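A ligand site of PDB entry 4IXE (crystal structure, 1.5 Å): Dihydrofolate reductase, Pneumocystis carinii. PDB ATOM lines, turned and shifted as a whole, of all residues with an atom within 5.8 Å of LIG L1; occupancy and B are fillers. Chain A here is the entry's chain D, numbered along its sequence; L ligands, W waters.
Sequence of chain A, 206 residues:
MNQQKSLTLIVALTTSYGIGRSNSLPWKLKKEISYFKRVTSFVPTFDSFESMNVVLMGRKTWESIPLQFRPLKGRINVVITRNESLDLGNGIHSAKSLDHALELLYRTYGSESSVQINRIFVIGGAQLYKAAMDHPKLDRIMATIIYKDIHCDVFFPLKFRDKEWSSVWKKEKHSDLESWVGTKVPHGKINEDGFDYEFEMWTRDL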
ATOM      1  N   ILE A  10     -19.065  -6.476   6.911  1.00  0.00           N
ATOM      2  CA  ILE A  10     -18.607  -5.073   7.181  1.00  0.00           C
ATOM      3  C   ILE A  10     -19.359  -4.217   6.158  1.00  0.00           C
ATOM      4  O   ILE A  10     -19.470  -4.568   4.981  1.00  0.00           O
ATOM      5  CB  ILE A  10     -17.035  -5.006   7.112  1.00  0.00           C
ATOM      6  CG1 ILE A  10     -16.627  -3.540   7.341  1.00  0.00           C
ATOM      7  CG2 ILE A  10     -16.501  -5.523   5.744  1.00  0.00           C
ATOM      8  CD1 ILE A  10     -15.130  -3.479   7.734  1.00  0.00           C
ATOM      9  N   VAL A  11     -19.863  -3.082   6.646  1.00  0.00           N
ATOM     10  CA  VAL A  11     -20.731  -2.206   5.858  1.00  0.00           C
ATOM     11  C   VAL A  11     -20.650  -0.748   6.351  1.00  0.00           C
ATOM     12  O   VAL A  11     -20.397  -0.524   7.525  1.00  0.00           O
ATOM     13  CB  VAL A  11     -22.256  -2.691   5.942  1.00  0.00           C
ATOM     14  CG1 VAL A  11     -22.807  -2.770   7.397  1.00  0.00           C
ATOM     15  CG2 VAL A  11     -23.146  -1.848   5.006  1.00  0.00           C
ATOM     16  N   ALA A  12     -20.845   0.209   5.463  1.00  0.00           N
ATOM     17  CA  ALA A  12     -21.043   1.605   5.834  1.00  0.00           C
ATOM     18  C   ALA A  12     -22.445   1.928   5.391  1.00  0.00           C
ATOM     19  O   ALA A  12     -22.835   1.656   4.226  1.00  0.00           O
ATOM     20  CB  ALA A  12     -20.038   2.480   5.007  1.00  0.00           C
ATOM     21  N   LEU A  25     -20.189   4.609  -3.643  1.00  0.00           N
ATOM     22  CA  LEU A  25     -20.553   5.066  -2.259  1.00  0.00           C
ATOM     23  C   LEU A  25     -20.658   6.571  -2.262  1.00  0.00           C
ATOM     24  O   LEU A  25     -19.659   7.235  -2.622  1.00  0.00           O
ATOM     25  CB  LEU A  25     -19.460   4.660  -1.294  1.00  0.00           C
ATOM     26  CG  LEU A  25     -19.174   3.176  -1.202  1.00  0.00           C
ATOM     27  CD1 LEU A  25     -18.312   2.890   0.000  1.00  0.00           C
ATOM     28  CD2 LEU A  25     -20.436   2.401  -0.967  1.00  0.00           C
ATOM     29  N   GLU A  32     -12.772   6.245   7.028  1.00  0.00           N
ATOM     30  CA  GLU A  32     -13.525   5.020   6.734  1.00  0.00           C
ATOM     31  C   GLU A  32     -12.688   4.141   5.824  1.00  0.00           C
ATOM     32  O   GLU A  32     -12.654   2.906   5.948  1.00  0.00           O
ATOM     33  CB  GLU A  32     -14.860   5.369   6.051  1.00  0.00           C
ATOM     34  CG  GLU A  32     -16.058   4.566   6.583  1.00  0.00           C
ATOM     35  CD  GLU A  32     -15.975   3.084   6.212  1.00  0.00           C
ATOM     36  OE1 GLU A  32     -15.822   2.773   5.003  1.00  0.00           O
ATOM     37  OE2 GLU A  32     -16.065   2.252   7.123  1.00  0.00           O
ATOM     38  N   TYR A  35     -10.026   2.456   7.896  1.00  0.00           N
ATOM     39  CA  TYR A  35     -10.655   1.493   8.784  1.00  0.00           C
ATOM     40  C   TYR A  35     -11.035   0.247   8.012  1.00  0.00           C
ATOM     41  O   TYR A  35     -10.692  -0.864   8.465  1.00  0.00           O
ATOM     42  CB  TYR A  35     -11.895   2.108   9.422  1.00  0.00           C
ATOM     43  CG  TYR A  35     -12.613   1.173  10.391  1.00  0.00           C
ATOM     44  CD1 TYR A  35     -12.152   1.002  11.701  1.00  0.00           C
ATOM     45  CD2 TYR A  35     -13.766   0.532   9.973  1.00  0.00           C
ATOM     46  CE1 TYR A  35     -12.821   0.201  12.568  1.00  0.00           C
ATOM     47  CE2 TYR A  35     -14.497  -0.321  10.828  1.00  0.00           C
ATOM     48  CZ  TYR A  35     -14.004  -0.465  12.137  1.00  0.00           C
ATOM     49  OH  TYR A  35     -14.649  -1.234  13.087  1.00  0.00           O
ATOM     50  N   PHE A  36     -11.634   0.410   6.833  1.00  0.00           N
ATOM     51  CA  PHE A  36     -11.988  -0.799   6.058  1.00  0.00           C
ATOM     52  C   PHE A  36     -10.748  -1.597   5.715  1.00  0.00           C
ATOM     53  O   PHE A  36     -10.740  -2.846   5.834  1.00  0.00           O
ATOM     54  CB  PHE A  36     -12.765  -0.360   4.811  1.00  0.00           C
ATOM     55  CG  PHE A  36     -13.008  -1.496   3.847  1.00  0.00           C
ATOM     56  CD1 PHE A  36     -14.116  -2.352   4.009  1.00  0.00           C
ATOM     57  CD2 PHE A  36     -12.134  -1.689   2.787  1.00  0.00           C
ATOM     58  CE1 PHE A  36     -14.311  -3.411   3.119  1.00  0.00           C
ATOM     59  CE2 PHE A  36     -12.320  -2.761   1.884  1.00  0.00           C
ATOM     60  CZ  PHE A  36     -13.433  -3.611   2.052  1.00  0.00           C
ATOM     61  N   THR A  61     -20.104  -5.192  -7.156  1.00  0.00           N
ATOM     62  CA  THR A  61     -19.103  -4.538  -6.293  1.00  0.00           C
ATOM     63  C   THR A  61     -17.689  -4.741  -6.863  1.00  0.00           C
ATOM     64  O   THR A  61     -16.836  -3.809  -6.893  1.00  0.00           O
ATOM     65  CB  THR A  61     -19.233  -5.001  -4.809  1.00  0.00           C
ATOM     66  OG1 THR A  61     -20.511  -4.627  -4.295  1.00  0.00           O
ATOM     67  CG2 THR A  61     -18.125  -4.462  -3.920  1.00  0.00           C
ATOM     68  N   SER A  64     -17.081  -2.447  -9.560  1.00  0.00           N
ATOM     69  CA  SER A  64     -16.987  -1.048  -9.077  1.00  0.00           C
ATOM     70  C   SER A  64     -15.608  -0.693  -8.509  1.00  0.00           C
ATOM     71  O   SER A  64     -15.299   0.494  -8.278  1.00  0.00           O
ATOM     72  CB  SER A  64     -18.114  -0.734  -8.081  1.00  0.00           C
ATOM     73  OG  SER A  64     -17.810  -1.119  -6.718  1.00  0.00           O
ATOM     74  N   ILE A  65     -14.770  -1.698  -8.273  1.00  0.00           N
ATOM     75  CA  ILE A  65     -13.461  -1.400  -7.782  1.00  0.00           C
ATOM     76  C   ILE A  65     -12.574  -1.008  -8.937  1.00  0.00           C
ATOM     77  O   ILE A  65     -12.461  -1.794  -9.873  1.00  0.00           O
ATOM     78  CB  ILE A  65     -12.845  -2.614  -7.051  1.00  0.00           C
ATOM     79  CG1 ILE A  65     -13.775  -2.955  -5.884  1.00  0.00           C
ATOM     80  CG2 ILE A  65     -11.459  -2.202  -6.504  1.00  0.00           C
ATOM     81  CD1 ILE A  65     -13.356  -4.264  -5.243  1.00  0.00           C
ATOM     82  N   PRO A  66     -11.901   0.161  -8.846  1.00  0.00           N
ATOM     83  CA  PRO A  66     -11.024   0.466 -10.001  1.00  0.00           C
ATOM     84  C   PRO A  66      -9.966  -0.618 -10.186  1.00  0.00           C
ATOM     85  O   PRO A  66      -9.412  -1.144  -9.222  1.00  0.00           O
ATOM     86  CB  PRO A  66     -10.344   1.788  -9.551  1.00  0.00           C
ATOM     87  CG  PRO A  66     -11.433   2.479  -8.775  1.00  0.00           C
ATOM     88  CD  PRO A  66     -11.950   1.306  -7.908  1.00  0.00           C
ATOM     89  N   PHE A  69      -6.855  -0.947  -8.017  1.00  0.00           N
ATOM     90  CA  PHE A  69      -6.986  -1.340  -6.608  1.00  0.00           C
ATOM     91  C   PHE A  69      -7.428  -2.806  -6.483  1.00  0.00           C
ATOM     92  O   PHE A  69      -7.786  -3.263  -5.337  1.00  0.00           O
ATOM     93  CB  PHE A  69      -8.023  -0.440  -5.929  1.00  0.00           C
ATOM     94  CG  PHE A  69      -7.664   1.030  -5.942  1.00  0.00           C
ATOM     95  CD1 PHE A  69      -6.387   1.441  -5.498  1.00  0.00           C
ATOM     96  CD2 PHE A  69      -8.585   2.002  -6.375  1.00  0.00           C
ATOM     97  CE1 PHE A  69      -6.028   2.790  -5.514  1.00  0.00           C
ATOM     98  CE2 PHE A  69      -8.222   3.361  -6.384  1.00  0.00           C
ATOM     99  CZ  PHE A  69      -6.949   3.738  -5.940  1.00  0.00           C
ATOM    100  N   LEU A  72      -8.127  -6.661  -3.995  1.00  0.00           N
ATOM    101  CA  LEU A  72      -7.790  -5.958  -2.732  1.00  0.00           C
ATOM    102  C   LEU A  72      -6.616  -6.648  -2.080  1.00  0.00           C
ATOM    103  O   LEU A  72      -6.700  -7.833  -1.671  1.00  0.00           O
ATOM    104  CB  LEU A  72      -9.012  -5.970  -1.796  1.00  0.00           C
ATOM    105  CG  LEU A  72     -10.228  -5.286  -2.391  1.00  0.00           C
ATOM    106  CD1 LEU A  72     -11.401  -5.380  -1.413  1.00  0.00           C
ATOM    107  CD2 LEU A  72      -9.964  -3.819  -2.691  1.00  0.00           C
ATOM    108  N   ARG A  75      -5.401  -9.784   0.998  1.00  0.00           N
ATOM    109  CA  ARG A  75      -6.624 -10.521   1.406  1.00  0.00           C
ATOM    110  C   ARG A  75      -6.927 -11.500   0.295  1.00  0.00           C
ATOM    111  O   ARG A  75      -6.661 -11.225  -0.864  1.00  0.00           O
ATOM    112  CB  ARG A  75      -7.816  -9.578   1.618  1.00  0.00           C
ATOM    113  CG  ARG A  75      -7.651  -8.722   2.899  1.00  0.00           C
ATOM    114  CD  ARG A  75      -8.335  -7.392   2.721  1.00  0.00           C
ATOM    115  NE  ARG A  75      -7.493  -6.533   1.881  1.00  0.00           N
ATOM    116  CZ  ARG A  75      -7.767  -5.261   1.625  1.00  0.00           C
ATOM    117  NH1 ARG A  75      -8.822  -4.674   2.108  1.00  0.00           N
ATOM    118  NH2 ARG A  75      -6.929  -4.542   0.847  1.00  0.00           N
ATOM    119  N   VAL A 122     -17.803 -10.446   4.472  1.00  0.00           N
ATOM    120  CA  VAL A 122     -18.690 -10.105   3.357  1.00  0.00           C
ATOM    121  C   VAL A 122     -18.655  -8.587   3.252  1.00  0.00           C
ATOM    122  O   VAL A 122     -18.957  -7.849   4.221  1.00  0.00           O
ATOM    123  CB  VAL A 122     -20.147 -10.625   3.615  1.00  0.00           C
ATOM    124  CG1 VAL A 122     -21.075 -10.081   2.485  1.00  0.00           C
ATOM    125  CG2 VAL A 122     -20.140 -12.170   3.765  1.00  0.00           C
ATOM    126  N   ILE A 123     -18.275  -8.122   2.031  1.00  0.00           N
ATOM    127  CA  ILE A 123     -17.997  -6.667   1.821  1.00  0.00           C
ATOM    128  C   ILE A 123     -18.970  -5.931   0.899  1.00  0.00           C
ATOM    129  O   ILE A 123     -18.736  -4.751   0.515  1.00  0.00           O
ATOM    130  CB  ILE A 123     -16.530  -6.387   1.427  1.00  0.00           C
ATOM    131  CG1 ILE A 123     -16.265  -6.816  -0.015  1.00  0.00           C
ATOM    132  CG2 ILE A 123     -15.545  -6.996   2.456  1.00  0.00           C
ATOM    133  CD1 ILE A 123     -15.012  -6.090  -0.605  1.00  0.00           C
ATOM    134  N   GLY A 124     -20.051  -6.637   0.542  1.00  0.00           N
ATOM    135  CA  GLY A 124     -21.155  -6.036  -0.208  1.00  0.00           C
ATOM    136  C   GLY A 124     -21.220  -6.689  -1.576  1.00  0.00           C
ATOM    137  O   GLY A 124     -20.500  -7.609  -1.887  1.00  0.00           O
ATOM    138  N   TYR A 129     -25.204  -8.899   0.610  1.00  0.00           N
ATOM    139  CA  TYR A 129     -25.587  -8.683   2.020  1.00  0.00           C
ATOM    140  C   TYR A 129     -26.925  -9.425   2.375  1.00  0.00           C
ATOM    141  O   TYR A 129     -27.051  -9.873   3.497  1.00  0.00           O
ATOM    142  CB  TYR A 129     -25.758  -7.244   2.366  1.00  0.00           C
ATOM    143  CG  TYR A 129     -24.475  -6.377   2.414  1.00  0.00           C
ATOM    144  CD1 TYR A 129     -23.305  -6.858   3.073  1.00  0.00           C
ATOM    145  CD2 TYR A 129     -24.517  -5.050   2.003  1.00  0.00           C
ATOM    146  CE1 TYR A 129     -22.129  -6.094   3.196  1.00  0.00           C
ATOM    147  CE2 TYR A 129     -23.364  -4.243   2.113  1.00  0.00           C
ATOM    148  CZ  TYR A 129     -22.202  -4.782   2.743  1.00  0.00           C
ATOM    149  OH  TYR A 129     -21.127  -3.874   2.782  1.00  0.00           O
ATOM    150  N   MET A 142     -19.659  -5.315  11.348  1.00  0.00           N
ATOM    151  CA  MET A 142     -18.812  -4.112  11.641  1.00  0.00           C
ATOM    152  C   MET A 142     -19.494  -2.996  10.813  1.00  0.00           C
ATOM    153  O   MET A 142     -19.440  -2.952   9.565  1.00  0.00           O
ATOM    154  CB  MET A 142     -17.395  -4.327  11.151  1.00  0.00           C
ATOM    155  CG  MET A 142     -16.706  -5.650  11.640  1.00  0.00           C
ATOM    156  SD  MET A 142     -16.633  -5.768  13.416  1.00  0.00           S
ATOM    157  CE  MET A 142     -15.272  -4.605  13.761  1.00  0.00           C
ATOM    158  N   THR A 144     -20.323   0.967   9.952  1.00  0.00           N
ATOM    159  CA  THR A 144     -20.001   2.396  10.070  1.00  0.00           C
ATOM    160  C   THR A 144     -21.278   3.136   9.865  1.00  0.00           C
ATOM    161  O   THR A 144     -21.830   3.097   8.738  1.00  0.00           O
ATOM    162  CB  THR A 144     -19.032   2.819   8.996  1.00  0.00           C
ATOM    163  OG1 THR A 144     -17.805   2.049   9.126  1.00  0.00           O
ATOM    164  CG2 THR A 144     -18.724   4.337   9.108  1.00  0.00           C
HETATM  165  C1  LIG L   1     -16.643  -1.591   0.866  1.00  0.00           C
HETATM  166  C2  LIG L   1     -16.866  -1.219   2.202  1.00  0.00           C
HETATM  167  C3  LIG L   1     -17.565  -2.029   3.186  1.00  0.00           C
HETATM  168  N1  LIG L   1     -18.070  -3.229   2.864  1.00  0.00           N
HETATM  169  N2  LIG L   1     -17.702  -1.638   4.439  1.00  0.00           N
HETATM  170  C4  LIG L   1     -17.168  -0.469   4.885  1.00  0.00           C
HETATM  171  N3  LIG L   1     -17.297  -0.080   6.161  1.00  0.00           N
HETATM  172  N4  LIG L   1     -16.453   0.322   4.049  1.00  0.00           N
HETATM  173  C5  LIG L   1     -16.316   0.006   2.700  1.00  0.00           C
HETATM  174  N5  LIG L   1     -15.602   0.844   1.914  1.00  0.00           N
HETATM  175  C6  LIG L   1     -15.432   0.496   0.608  1.00  0.00           C
HETATM  176  C7  LIG L   1     -15.912  -0.668   0.051  1.00  0.00           C
HETATM  177  N6  LIG L   1     -15.641  -0.946  -1.264  1.00  0.00           N
HETATM  178  C8  LIG L   1     -16.569  -1.777  -2.048  1.00  0.00           C
HETATM  179  C9  LIG L   1     -14.474  -0.576  -1.875  1.00  0.00           C
HETATM  180  C10 LIG L   1     -14.542  -0.049  -3.186  1.00  0.00           C
HETATM  181  C11 LIG L   1     -13.276   0.259  -3.702  1.00  0.00           C
HETATM  182  F1  LIG L   1     -13.118   0.812  -5.059  1.00  0.00           F
HETATM  183  C12 LIG L   1     -12.072   0.035  -3.008  1.00  0.00           C
HETATM  184  F2  LIG L   1     -10.743   0.341  -3.605  1.00  0.00           F
HETATM  185  C13 LIG L   1     -12.041  -0.447  -1.757  1.00  0.00           C
HETATM  186  F3  LIG L   1     -10.824  -0.632  -1.062  1.00  0.00           F
HETATM  187  C14 LIG L   1     -13.257  -0.789  -1.215  1.00  0.00           C
HETATM  188  P1  LG2 L   2     -23.611  -6.862  -5.645  1.00  0.00           P
HETATM  189  O1  LG2 L   2     -24.289  -7.598  -4.623  1.00  0.00           O
HETATM  190  O2  LG2 L   2     -22.227  -6.336  -5.420  1.00  0.00           O
HETATM  191  O3  LG2 L   2     -23.525  -7.590  -7.029  1.00  0.00           O
HETATM  192  C1  LG2 L   2     -24.703  -8.269  -7.509  1.00  0.00           C
HETATM  193  C2  LG2 L   2     -24.295  -9.396  -8.429  1.00  0.00           C
HETATM  194  O4  LG2 L   2     -23.511 -10.297  -7.615  1.00  0.00           O
HETATM  195  C3  LG2 L   2     -25.504 -10.268  -8.845  1.00  0.00           C
HETATM  196  O5  LG2 L   2     -26.071  -9.714 -10.066  1.00  0.00           O
HETATM  197  C4  LG2 L   2     -24.848 -11.604  -9.049  1.00  0.00           C
HETATM  198  O6  LG2 L   2     -23.893 -11.585 -10.070  1.00  0.00           O
HETATM  199  C5  LG2 L   2     -23.986 -11.610  -7.761  1.00  0.00           C
HETATM  200  N1  LG2 L   2     -24.640 -12.022  -6.549  1.00  0.00           N
HETATM  201  C6  LG2 L   2     -24.886 -11.290  -5.430  1.00  0.00           C
HETATM  202  N2  LG2 L   2     -25.420 -12.077  -4.521  1.00  0.00           N
HETATM  203  C7  LG2 L   2     -25.443 -13.333  -5.065  1.00  0.00           C
HETATM  204  C8  LG2 L   2     -25.878 -14.501  -4.521  1.00  0.00           C
HETATM  205  N3  LG2 L   2     -26.326 -14.511  -3.256  1.00  0.00           N
HETATM  206  N4  LG2 L   2     -25.805 -15.653  -5.201  1.00  0.00           N
HETATM  207  C9  LG2 L   2     -25.292 -15.614  -6.460  1.00  0.00           C
HETATM  208  N5  LG2 L   2     -24.864 -14.395  -7.065  1.00  0.00           N
HETATM  209  C10 LG2 L   2     -24.967 -13.285  -6.282  1.00  0.00           C
HETATM  210  O7  LG2 L   2     -24.551  -5.546  -6.144  1.00  0.00           O
HETATM  211  P2  LG2 L   2     -25.765  -4.755  -5.672  1.00  0.00           P
HETATM  212  O8  LG2 L   2     -26.717  -5.385  -4.747  1.00  0.00           O
HETATM  213  O9  LG2 L   2     -26.187  -4.200  -7.043  1.00  0.00           O
HETATM  214  O10 LG2 L   2     -25.104  -3.609  -4.852  1.00  0.00           O
HETATM  215  C11 LG2 L   2     -24.176  -2.690  -5.473  1.00  0.00           C
HETATM  216  C12 LG2 L   2     -24.269  -1.384  -4.658  1.00  0.00           C
HETATM  217  O11 LG2 L   2     -23.832  -1.621  -3.329  1.00  0.00           O
HETATM  218  C13 LG2 L   2     -23.363  -0.310  -5.194  1.00  0.00           C
HETATM  219  O12 LG2 L   2     -23.971   1.032  -5.074  1.00  0.00           O
HETATM  220  C14 LG2 L   2     -22.212  -0.339  -4.250  1.00  0.00           C
HETATM  221  O13 LG2 L   2     -21.494   0.922  -4.303  1.00  0.00           O
HETATM  222  C15 LG2 L   2     -22.943  -0.585  -2.943  1.00  0.00           C
HETATM  223  N6  LG2 L   2     -22.027  -1.117  -1.967  1.00  0.00           N
HETATM  224  C16 LG2 L   2     -22.061  -0.528  -0.677  1.00  0.00           C
HETATM  225  C17 LG2 L   2     -21.220  -0.982   0.338  1.00  0.00           C
HETATM  226  C18 LG2 L   2     -21.348  -0.366   1.608  1.00  0.00           C
HETATM  227  O14 LG2 L   2     -20.818  -0.883   2.611  1.00  0.00           O
HETATM  228  N7  LG2 L   2     -21.940   0.829   1.714  1.00  0.00           N
HETATM  229  C19 LG2 L   2     -20.235  -2.001   0.093  1.00  0.00           C
HETATM  230  C20 LG2 L   2     -20.232  -2.585  -1.226  1.00  0.00           C
HETATM  231  C21 LG2 L   2     -21.098  -2.147  -2.246  1.00  0.00           C
HETATM  232  P3  LG2 L   2     -24.154 -12.061 -11.665  1.00  0.00           P
HETATM  233  O15 LG2 L   2     -24.699 -13.422 -11.550  1.00  0.00           O
HETATM  234  O16 LG2 L   2     -25.229 -11.054 -12.125  1.00  0.00           O
HETATM  235  O17 LG2 L   2     -22.853 -11.846 -12.337  1.00  0.00           O
HETATM  236  O   HOH W   1     -13.844   2.739   2.825  1.00  0.00           O
HETATM  237  O   HOH W   2     -17.628  -0.733   9.546  1.00  0.00           O
HETATM  238  O   HOH W   3      -8.876  -1.839   1.316  1.00  0.00           O
HETATM  239  O   HOH W   4     -11.986   1.837   0.974  1.00  0.00           O
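A nitrogen (N4) of LIG L1 sits at hydrogen-bond distance from the side-chain carboxylate (OE1) of Glu 32.
N1 of LIG L1 lies within hydrogen-bond range of O of Ile 10 (2.9 Å).
N1 of LIG L1 sits at hydrogen-bond distance from O of Ile 123 (2.9 Å).
The side-chain hydroxyl (OH) of Tyr 129 lies within hydrogen-bond range of a nitrogen (N1) of LIG L1.
A nitrogen (N2) of LIG L1 lies close to the backbone NH of Val 11 (3.4 Å).
O of Val 11 is in hydrogen-bond range of N3 of LIG L1.
OH of Tyr 129 lies within hydrogen-bond range of O14 of LG2 L2 (3.0 Å).
The backbone NH of Thr 61 lies within hydrogen-bond range of an oxygen (O2) of LG2 L2 (3.0 Å).
An oxygen (O2) of LG2 L2 sits at hydrogen-bond distance from the side-chain hydroxyl (OG1) of Thr 61.
N of Ala 12 lies within hydrogen-bond range of O14 of LG2 L2, 3.1 Å away.
O of Ala 12 is in hydrogen-bond range of N7 of LG2 L2 (2.8 Å).
The side-chain carboxylate of Glu 32 sits at hydrogen-bond distance from the side-chain hydroxyl of Thr 144, 2.7 Å away.
The backbone carbonyl oxygen of Ile 10 is in hydrogen-bond range of the side-chain hydroxyl of Tyr 129, 2.8 Å away.
The backbone NH of Ile 10 lies within hydrogen-bond range of the backbone carbonyl oxygen of Val 122, at 3.0 Å.
The side-chain hydroxyl (OH) of Tyr 129 sits at hydrogen-bond distance from the backbone carbonyl oxygen (O) of Ile 123.
N of Thr 144 lies within hydrogen-bond range of O of Val 11 (2.8 Å).
N of Val 11 sits at hydrogen-bond distance from O of Met 142, 3.0 Å away.
O of Thr 61 lies within hydrogen-bond range of OG of Ser 64.
Merely in contact with LIG L1: Pro 66 (3.1 Å), Phe 36 (3.5 Å), Ile 65 (3.5 Å), Thr 61 (3.6 Å), Ala 12 (3.6 Å), Phe 69 (3.7 Å), Leu 72 (3.7 Å), Thr 144 (3.7 Å), Leu 25 (3.8 Å) and Ser 64 (3.9 Å).
Hydrophobic or aromatic side chains that line LIG L1: Ile 10, Ala 12, Leu 25, Phe 36, Ile 65, Pro 66, Phe 69, Leu 72 and Ile 123.
Water W1 lies within hydrogen-bond range of N5 of LIG L1 (2.7 Å) and OE1 of Glu 32 (2.9 Å).
Water W2 lies within hydrogen-bond range of OG1 of Thr 144 (2.8 Å), O of Met 142 (2.9 Å), O of Val 11 (3.4 Å) and N3 of LIG L1 (3.5 Å).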
